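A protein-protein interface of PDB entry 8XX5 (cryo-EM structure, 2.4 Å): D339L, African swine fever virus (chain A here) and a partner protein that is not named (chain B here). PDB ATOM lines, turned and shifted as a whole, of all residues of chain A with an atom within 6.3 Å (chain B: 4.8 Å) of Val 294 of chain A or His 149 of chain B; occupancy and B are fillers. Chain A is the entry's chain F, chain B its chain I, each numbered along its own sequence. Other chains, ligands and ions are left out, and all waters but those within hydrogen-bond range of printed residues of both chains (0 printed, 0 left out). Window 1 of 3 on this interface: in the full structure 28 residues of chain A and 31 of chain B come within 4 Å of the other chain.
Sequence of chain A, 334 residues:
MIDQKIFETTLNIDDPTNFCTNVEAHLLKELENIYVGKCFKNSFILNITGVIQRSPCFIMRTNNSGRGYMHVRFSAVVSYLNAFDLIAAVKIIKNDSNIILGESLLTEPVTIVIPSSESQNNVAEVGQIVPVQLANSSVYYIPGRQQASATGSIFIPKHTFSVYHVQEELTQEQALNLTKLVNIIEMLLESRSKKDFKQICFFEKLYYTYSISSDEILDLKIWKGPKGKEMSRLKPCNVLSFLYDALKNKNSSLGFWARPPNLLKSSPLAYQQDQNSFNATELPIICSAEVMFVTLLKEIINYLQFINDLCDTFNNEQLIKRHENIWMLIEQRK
Printed residues of chain B that touch a printed residue of chain A: Phe 102, Phe 143, Gly 147, Gly 148, His 149, Trp 151 and Leu 152. Hydrophobic or aromatic side chains of chain B that line the printed part of chain A: Phe 102, Phe 143, Trp 151 and Leu 152. Along chain B the printed residues that touch a printed residue of chain A span positions 102 to 152. Hydrophobic or aromatic side chains of chain A within 4 Å of the printed part of chain B: Leu 181, Val 291 and Val 294. Among the printed residues, 12 pairs touch across the chains. Among the printed residues, no Asp or Glu carboxylate lies within 4 Å of a Lys or Arg side-chain nitrogen of the other chain.
The backbone carbonyl oxygen of Gly 147 of chain B sits at hydrogen-bond distance from the side-chain amino group of Lys 298 of chain A (3.5 Å).
Of chain B, only Gly 148 (3.4 Å), His 149 (3.9 Å) and Leu 152 (3.97 Å) come within 4 Å of Val 294 of chain A. Of chain A, only Val 294 (3.9 Å) comes within 4 Å of His 149 of chain B. Of the printed residues of chain B, Asn 177 of chain A touches Trp 151 and Leu 152. Of the printed residues of chain A, Phe 143 of chain B touches Val 291. Printed residues of chain A within 4 Å of Gly 147 of chain B: Lys 298 (3.5 Å). Printed residues of chain A within 4 Å of Trp 151 of chain B: Asn 177 and Leu 181. Of the printed residues of chain B, Leu 181 of chain A touches Trp 151. Gly 91 of chain B touches none of the printed residues of chain A.
The backbone carbonyl oxygen (O) of Phe 143 of chain B lies within hydrogen-bond range of the side-chain hydroxyl (OG) of Ser 146 of chain B (2.6 Å). The backbone NH of His 149 of chain B is in hydrogen-bond range of the side-chain hydroxyl of Ser 146 of chain B (3.4 Å). The backbone carbonyl oxygen (O) of Val 291 of chain A sits at hydrogen-bond distance from the side-chain hydroxyl (OG1) of Thr 295 of chain A (2.5 Å).
Among the printed residues, merely in contact across the chains: Asn 177 of chain A with Trp 151 of chain B, Asn 177 of chain A with Leu 152 of chain B, Leu 181 of chain A with Trp 151 of chain B, Glu 290 of chain A with Phe 102 of chain B, Glu 290 of chain A with Leu 152 of chain B, Val 291 of chain A with Phe 102 of chain B, Val 291 of chain A with Phe 143 of chain B, Val 294 of chain A with Gly 148 of chain B, Val 294 of chain A with His 149 of chain B, Val 294 of chain A with Leu 152 of chain B and Lys 298 of chain A with Gly 148 of chain B.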
ATOM      1  N   ASN A 177      17.930  20.518  -3.021  1.00  0.00           N
ATOM      2  CA  ASN A 177      16.793  19.882  -3.679  1.00  0.00           C
ATOM      3  C   ASN A 177      16.689  18.409  -3.299  1.00  0.00           C
ATOM      4  O   ASN A 177      15.588  17.899  -3.063  1.00  0.00           O
ATOM      5  CB  ASN A 177      16.905  20.042  -5.194  1.00  0.00           C
ATOM      6  CG  ASN A 177      15.559  19.968  -5.888  1.00  0.00           C
ATOM      7  OD1 ASN A 177      15.319  19.083  -6.708  1.00  0.00           O
ATOM      8  ND2 ASN A 177      14.672  20.897  -5.556  1.00  0.00           N
ATOM      9  N   LEU A 178      17.825  17.709  -3.240  1.00  0.00           N
ATOM     10  CA  LEU A 178      17.828  16.311  -2.818  1.00  0.00           C
ATOM     11  C   LEU A 178      17.419  16.150  -1.360  1.00  0.00           C
ATOM     12  O   LEU A 178      16.989  15.060  -0.961  1.00  0.00           O
ATOM     13  CB  LEU A 178      19.211  15.695  -3.035  1.00  0.00           C
ATOM     14  CG  LEU A 178      19.661  15.475  -4.478  1.00  0.00           C
ATOM     15  CD1 LEU A 178      21.159  15.699  -4.613  1.00  0.00           C
ATOM     16  CD2 LEU A 178      19.283  14.080  -4.934  1.00  0.00           C
ATOM     17  N   LEU A 181      13.953  14.655  -0.994  1.00  0.00           N
ATOM     18  CA  LEU A 181      13.878  13.201  -1.071  1.00  0.00           C
ATOM     19  C   LEU A 181      14.486  12.547   0.160  1.00  0.00           C
ATOM     20  O   LEU A 181      14.027  11.485   0.591  1.00  0.00           O
ATOM     21  CB  LEU A 181      14.576  12.697  -2.334  1.00  0.00           C
ATOM     22  CG  LEU A 181      13.963  13.088  -3.675  1.00  0.00           C
ATOM     23  CD1 LEU A 181      14.874  12.661  -4.814  1.00  0.00           C
ATOM     24  CD2 LEU A 181      12.580  12.481  -3.825  1.00  0.00           C
ATOM     25  N   ALA A 289      26.418  13.966 -10.397  1.00  0.00           N
ATOM     26  CA  ALA A 289      26.075  13.486  -9.064  1.00  0.00           C
ATOM     27  C   ALA A 289      24.585  13.616  -8.795  1.00  0.00           C
ATOM     28  O   ALA A 289      23.998  12.755  -8.130  1.00  0.00           O
ATOM     29  CB  ALA A 289      26.878  14.246  -8.009  1.00  0.00           C
ATOM     30  N   GLU A 290      23.958  14.680  -9.302  1.00  0.00           N
ATOM     31  CA  GLU A 290      22.528  14.868  -9.086  1.00  0.00           C
ATOM     32  C   GLU A 290      21.713  13.756  -9.732  1.00  0.00           C
ATOM     33  O   GLU A 290      20.765  13.248  -9.129  1.00  0.00           O
ATOM     34  CB  GLU A 290      22.088  16.225  -9.625  1.00  0.00           C
ATOM     35  CG  GLU A 290      21.071  16.924  -8.748  1.00  0.00           C
ATOM     36  CD  GLU A 290      19.675  16.369  -8.910  1.00  0.00           C
ATOM     37  OE1 GLU A 290      19.354  15.864 -10.005  1.00  0.00           O
ATOM     38  OE2 GLU A 290      18.894  16.451  -7.939  1.00  0.00           O
ATOM     39  N   VAL A 291      22.067  13.366 -10.958  1.00  0.00           N
ATOM     40  CA  VAL A 291      21.307  12.333 -11.658  1.00  0.00           C
ATOM     41  C   VAL A 291      21.385  11.012 -10.902  1.00  0.00           C
ATOM     42  O   VAL A 291      20.365  10.360 -10.644  1.00  0.00           O
ATOM     43  CB  VAL A 291      21.814  12.183 -13.103  1.00  0.00           C
ATOM     44  CG1 VAL A 291      21.178  10.973 -13.766  1.00  0.00           C
ATOM     45  CG2 VAL A 291      21.535  13.447 -13.898  1.00  0.00           C
ATOM     46  N   MET A 292      22.600  10.605 -10.529  1.00  0.00           N
ATOM     47  CA  MET A 292      22.774   9.349  -9.807  1.00  0.00           C
ATOM     48  C   MET A 292      22.084   9.388  -8.453  1.00  0.00           C
ATOM     49  O   MET A 292      21.422   8.421  -8.058  1.00  0.00           O
ATOM     50  CB  MET A 292      24.262   9.043  -9.635  1.00  0.00           C
ATOM     51  CG  MET A 292      24.545   7.835  -8.753  1.00  0.00           C
ATOM     52  SD  MET A 292      24.834   8.272  -7.026  1.00  0.00           S
ATOM     53  CE  MET A 292      25.987   9.629  -7.200  1.00  0.00           C
ATOM     54  N   PHE A 293      22.242  10.491  -7.717  1.00  0.00           N
ATOM     55  CA  PHE A 293      21.630  10.585  -6.399  1.00  0.00           C
ATOM     56  C   PHE A 293      20.113  10.551  -6.494  1.00  0.00           C
ATOM     57  O   PHE A 293      19.451   9.887  -5.692  1.00  0.00           O
ATOM     58  CB  PHE A 293      22.102  11.853  -5.688  1.00  0.00           C
ATOM     59  CG  PHE A 293      23.400  11.685  -4.949  1.00  0.00           C
ATOM     60  CD1 PHE A 293      23.642  10.546  -4.200  1.00  0.00           C
ATOM     61  CD2 PHE A 293      24.374  12.668  -4.999  1.00  0.00           C
ATOM     62  CE1 PHE A 293      24.833  10.387  -3.519  1.00  0.00           C
ATOM     63  CE2 PHE A 293      25.568  12.514  -4.318  1.00  0.00           C
ATOM     64  CZ  PHE A 293      25.798  11.373  -3.578  1.00  0.00           C
ATOM     65  N   VAL A 294      19.543  11.247  -7.481  1.00  0.00           N
ATOM     66  CA  VAL A 294      18.097  11.234  -7.671  1.00  0.00           C
ATOM     67  C   VAL A 294      17.614   9.833  -8.019  1.00  0.00           C
ATOM     68  O   VAL A 294      16.604   9.360  -7.485  1.00  0.00           O
ATOM     69  CB  VAL A 294      17.699  12.261  -8.747  1.00  0.00           C
ATOM     70  CG1 VAL A 294      16.414  11.853  -9.429  1.00  0.00           C
ATOM     71  CG2 VAL A 294      17.543  13.629  -8.126  1.00  0.00           C
ATOM     72  N   THR A 295      18.330   9.142  -8.910  1.00  0.00           N
ATOM     73  CA  THR A 295      17.929   7.790  -9.287  1.00  0.00           C
ATOM     74  C   THR A 295      17.965   6.851  -8.087  1.00  0.00           C
ATOM     75  O   THR A 295      17.012   6.100  -7.838  1.00  0.00           O
ATOM     76  CB  THR A 295      18.835   7.269 -10.403  1.00  0.00           C
ATOM     77  OG1 THR A 295      19.114   8.327 -11.328  1.00  0.00           O
ATOM     78  CG2 THR A 295      18.165   6.121 -11.140  1.00  0.00           C
ATOM     79  N   LEU A 296      19.058   6.892  -7.322  1.00  0.00           N
ATOM     80  CA  LEU A 296      19.185   6.013  -6.164  1.00  0.00           C
ATOM     81  C   LEU A 296      18.140   6.337  -5.106  1.00  0.00           C
ATOM     82  O   LEU A 296      17.552   5.429  -4.507  1.00  0.00           O
ATOM     83  CB  LEU A 296      20.592   6.114  -5.576  1.00  0.00           C
ATOM     84  CG  LEU A 296      21.746   5.637  -6.460  1.00  0.00           C
ATOM     85  CD1 LEU A 296      23.003   5.435  -5.631  1.00  0.00           C
ATOM     86  CD2 LEU A 296      21.379   4.365  -7.206  1.00  0.00           C
ATOM     87  N   LEU A 297      17.891   7.626  -4.861  1.00  0.00           N
ATOM     88  CA  LEU A 297      16.913   8.008  -3.852  1.00  0.00           C
ATOM     89  C   LEU A 297      15.506   7.601  -4.266  1.00  0.00           C
ATOM     90  O   LEU A 297      14.712   7.163  -3.429  1.00  0.00           O
ATOM     91  CB  LEU A 297      16.985   9.511  -3.595  1.00  0.00           C
ATOM     92  CG  LEU A 297      18.181  10.005  -2.777  1.00  0.00           C
ATOM     93  CD1 LEU A 297      17.860  11.329  -2.103  1.00  0.00           C
ATOM     94  CD2 LEU A 297      18.650   8.969  -1.767  1.00  0.00           C
ATOM     95  N   LYS A 298      15.177   7.743  -5.553  1.00  0.00           N
ATOM     96  CA  LYS A 298      13.873   7.298  -6.029  1.00  0.00           C
ATOM     97  C   LYS A 298      13.732   5.787  -5.910  1.00  0.00           C
ATOM     98  O   LYS A 298      12.661   5.287  -5.555  1.00  0.00           O
ATOM     99  CB  LYS A 298      13.653   7.750  -7.471  1.00  0.00           C
ATOM    100  CG  LYS A 298      12.278   7.406  -8.020  1.00  0.00           C
ATOM    101  CD  LYS A 298      11.189   8.205  -7.326  1.00  0.00           C
ATOM    102  CE  LYS A 298       9.812   7.621  -7.607  1.00  0.00           C
ATOM    103  NZ  LYS A 298       8.918   8.593  -8.292  1.00  0.00           N
ATOM    104  N   GLU A 299      14.803   5.042  -6.202  1.00  0.00           N
ATOM    105  CA  GLU A 299      14.761   3.593  -6.018  1.00  0.00           C
ATOM    106  C   GLU A 299      14.539   3.229  -4.554  1.00  0.00           C
ATOM    107  O   GLU A 299      13.736   2.343  -4.235  1.00  0.00           O
ATOM    108  CB  GLU A 299      16.055   2.969  -6.540  1.00  0.00           C
ATOM    109  CG  GLU A 299      16.193   1.483  -6.264  1.00  0.00           C
ATOM    110  CD  GLU A 299      16.490   0.680  -7.515  1.00  0.00           C
ATOM    111  OE1 GLU A 299      16.118   1.133  -8.618  1.00  0.00           O
ATOM    112  OE2 GLU A 299      17.097  -0.404  -7.396  1.00  0.00           O
ATOM    113  N   PRO B  87       6.441  14.804 -17.954  1.00  0.00           N
ATOM    114  CA  PRO B  87       7.736  15.186 -17.368  1.00  0.00           C
ATOM    115  C   PRO B  87       8.904  15.079 -18.331  1.00  0.00           C
ATOM    116  O   PRO B  87       9.901  15.786 -18.148  1.00  0.00           O
ATOM    117  CB  PRO B  87       7.887  14.215 -16.187  1.00  0.00           C
ATOM    118  CG  PRO B  87       6.927  13.106 -16.461  1.00  0.00           C
ATOM    119  CD  PRO B  87       5.787  13.727 -17.195  1.00  0.00           C
ATOM    120  N   GLY B  91      11.208  18.256 -18.810  1.00  0.00           N
ATOM    121  CA  GLY B  91      12.631  18.180 -18.524  1.00  0.00           C
ATOM    122  C   GLY B  91      13.488  18.518 -19.726  1.00  0.00           C
ATOM    123  O   GLY B  91      14.539  19.145 -19.589  1.00  0.00           O
ATOM    124  N   PHE B 102      20.584  18.379 -17.560  1.00  0.00           N
ATOM    125  CA  PHE B 102      20.674  16.927 -17.691  1.00  0.00           C
ATOM    126  C   PHE B 102      21.101  16.511 -19.092  1.00  0.00           C
ATOM    127  O   PHE B 102      21.860  15.549 -19.250  1.00  0.00           O
ATOM    128  CB  PHE B 102      19.344  16.283 -17.313  1.00  0.00           C
ATOM    129  CG  PHE B 102      18.914  16.580 -15.909  1.00  0.00           C
ATOM    130  CD1 PHE B 102      19.811  16.464 -14.862  1.00  0.00           C
ATOM    131  CD2 PHE B 102      17.618  16.975 -15.635  1.00  0.00           C
ATOM    132  CE1 PHE B 102      19.424  16.737 -13.566  1.00  0.00           C
ATOM    133  CE2 PHE B 102      17.225  17.249 -14.342  1.00  0.00           C
ATOM    134  CZ  PHE B 102      18.129  17.130 -13.306  1.00  0.00           C
ATOM    135  N   PHE B 143      16.278   8.390 -18.307  1.00  0.00           N
ATOM    136  CA  PHE B 143      16.261   9.189 -17.087  1.00  0.00           C
ATOM    137  C   PHE B 143      15.177  10.256 -17.139  1.00  0.00           C
ATOM    138  O   PHE B 143      14.482  10.492 -16.145  1.00  0.00           O
ATOM    139  CB  PHE B 143      17.631   9.827 -16.865  1.00  0.00           C
ATOM    140  CG  PHE B 143      17.651  10.872 -15.787  1.00  0.00           C
ATOM    141  CD1 PHE B 143      17.352  10.541 -14.475  1.00  0.00           C
ATOM    142  CD2 PHE B 143      17.975  12.185 -16.083  1.00  0.00           C
ATOM    143  CE1 PHE B 143      17.373  11.501 -13.483  1.00  0.00           C
ATOM    144  CE2 PHE B 143      17.996  13.149 -15.094  1.00  0.00           C
ATOM    145  CZ  PHE B 143      17.695  12.806 -13.793  1.00  0.00           C
ATOM    146  N   LEU B 144      15.015  10.910 -18.292  1.00  0.00           N
ATOM    147  CA  LEU B 144      14.000  11.952 -18.413  1.00  0.00           C
ATOM    148  C   LEU B 144      12.597  11.388 -18.242  1.00  0.00           C
ATOM    149  O   LEU B 144      11.693  12.099 -17.789  1.00  0.00           O
ATOM    150  CB  LEU B 144      14.131  12.663 -19.760  1.00  0.00           C
ATOM    151  CG  LEU B 144      15.416  13.467 -19.968  1.00  0.00           C
ATOM    152  CD1 LEU B 144      15.528  13.948 -21.404  1.00  0.00           C
ATOM    153  CD2 LEU B 144      15.484  14.636 -19.006  1.00  0.00           C
ATOM    154  N   SER B 146      12.149   8.752 -16.253  1.00  0.00           N
ATOM    155  CA  SER B 146      12.210   8.025 -14.996  1.00  0.00           C
ATOM    156  C   SER B 146      11.425   8.752 -13.907  1.00  0.00           C
ATOM    157  O   SER B 146      11.097   9.935 -14.023  1.00  0.00           O
ATOM    158  CB  SER B 146      13.660   7.841 -14.553  1.00  0.00           C
ATOM    159  OG  SER B 146      14.189   9.051 -14.042  1.00  0.00           O
ATOM    160  N   GLY B 147      11.129   8.017 -12.835  1.00  0.00           N
ATOM    161  CA  GLY B 147      10.378   8.600 -11.734  1.00  0.00           C
ATOM    162  C   GLY B 147      11.143   9.687 -11.004  1.00  0.00           C
ATOM    163  O   GLY B 147      10.555  10.672 -10.551  1.00  0.00           O
ATOM    164  N   GLY B 148      12.459   9.522 -10.869  1.00  0.00           N
ATOM    165  CA  GLY B 148      13.240  10.510 -10.141  1.00  0.00           C
ATOM    166  C   GLY B 148      13.279  11.856 -10.842  1.00  0.00           C
ATOM    167  O   GLY B 148      13.028  12.900 -10.228  1.00  0.00           O
ATOM    168  N   HIS B 149      13.582  11.853 -12.140  1.00  0.00           N
ATOM    169  CA  HIS B 149      13.551  13.105 -12.884  1.00  0.00           C
ATOM    170  C   HIS B 149      12.135  13.641 -13.007  1.00  0.00           C
ATOM    171  O   HIS B 149      11.944  14.857 -13.083  1.00  0.00           O
ATOM    172  CB  HIS B 149      14.163  12.932 -14.272  1.00  0.00           C
ATOM    173  CG  HIS B 149      13.935  14.103 -15.174  1.00  0.00           C
ATOM    174  ND1 HIS B 149      14.725  15.232 -15.141  1.00  0.00           N
ATOM    175  CD2 HIS B 149      12.994  14.330 -16.120  1.00  0.00           C
ATOM    176  CE1 HIS B 149      14.286  16.100 -16.035  1.00  0.00           C
ATOM    177  NE2 HIS B 149      13.237  15.577 -16.644  1.00  0.00           N
ATOM    178  N   SER B 150      11.134  12.760 -13.040  1.00  0.00           N
ATOM    179  CA  SER B 150       9.752  13.226 -13.044  1.00  0.00           C
ATOM    180  C   SER B 150       9.448  14.015 -11.779  1.00  0.00           C
ATOM    181  O   SER B 150       8.872  15.107 -11.836  1.00  0.00           O
ATOM    182  CB  SER B 150       8.797  12.042 -13.184  1.00  0.00           C
ATOM    183  OG  SER B 150       7.519  12.358 -12.667  1.00  0.00           O
ATOM    184  N   TRP B 151       9.855  13.484 -10.625  1.00  0.00           N
ATOM    185  CA  TRP B 151       9.686  14.215  -9.375  1.00  0.00           C
ATOM    186  C   TRP B 151      10.456  15.527  -9.402  1.00  0.00           C
ATOM    187  O   TRP B 151       9.939  16.566  -8.975  1.00  0.00           O
ATOM    188  CB  TRP B 151      10.142  13.356  -8.194  1.00  0.00           C
ATOM    189  CG  TRP B 151      10.279  14.131  -6.916  1.00  0.00           C
ATOM    190  CD1 TRP B 151       9.313  14.343  -5.981  1.00  0.00           C
ATOM    191  CD2 TRP B 151      11.450  14.810  -6.443  1.00  0.00           C
ATOM    192  NE1 TRP B 151       9.808  15.104  -4.952  1.00  0.00           N
ATOM    193  CE2 TRP B 151      11.117  15.407  -5.214  1.00  0.00           C
ATOM    194  CE3 TRP B 151      12.746  14.969  -6.940  1.00  0.00           C
ATOM    195  CZ2 TRP B 151      12.032  16.150  -4.473  1.00  0.00           C
ATOM    196  CZ3 TRP B 151      13.651  15.712  -6.207  1.00  0.00           C
ATOM    197  CH2 TRP B 151      13.290  16.292  -4.986  1.00  0.00           C
ATOM    198  N   LEU B 152      11.692  15.501  -9.903  1.00  0.00           N
ATOM    199  CA  LEU B 152      12.509  16.710  -9.911  1.00  0.00           C
ATOM    200  C   LEU B 152      11.878  17.796 -10.776  1.00  0.00           C
ATOM    201  O   LEU B 152      11.786  18.958 -10.366  1.00  0.00           O
ATOM    202  CB  LEU B 152      13.921  16.386 -10.395  1.00  0.00           C
ATOM    203  CG  LEU B 152      14.942  17.523 -10.312  1.00  0.00           C
ATOM    204  CD1 LEU B 152      16.267  17.002  -9.792  1.00  0.00           C
ATOM    205  CD2 LEU B 152      15.125  18.212 -11.657  1.00  0.00           C
ATOM    206  N   ILE B 153      11.423  17.430 -11.975  1.00  0.00           N
ATOM    207  CA  ILE B 153      10.866  18.416 -12.891  1.00  0.00           C
ATOM    208  C   ILE B 153       9.498  18.892 -12.420  1.00  0.00           C
ATOM    209  O   ILE B 153       9.160  20.070 -12.581  1.00  0.00           O
ATOM    210  CB  ILE B 153      10.837  17.857 -14.329  1.00  0.00           C
ATOM    211  CG1 ILE B 153      11.109  18.979 -15.329  1.00  0.00           C
ATOM    212  CG2 ILE B 153       9.524  17.154 -14.644  1.00  0.00           C
ATOM    213  CD1 ILE B 153      12.420  19.686 -15.096  1.00  0.00           C
ATOM    214  N   ASN B 154       8.693  18.009 -11.819  1.00  0.00           N
ATOM    215  CA  ASN B 154       7.413  18.451 -11.282  1.00  0.00           C
ATOM    216  C   ASN B 154       7.617  19.401 -10.112  1.00  0.00           C
ATOM    217  O   ASN B 154       6.912  20.409  -9.996  1.00  0.00           O
ATOM    218  CB  ASN B 154       6.572  17.244 -10.871  1.00  0.00           C
ATOM    219  CG  ASN B 154       6.054  16.463 -12.064  1.00  0.00           C
ATOM    220  OD1 ASN B 154       5.996  16.981 -13.178  1.00  0.00           O
ATOM    221  ND2 ASN B 154       5.675  15.212 -11.835  1.00  0.00           N
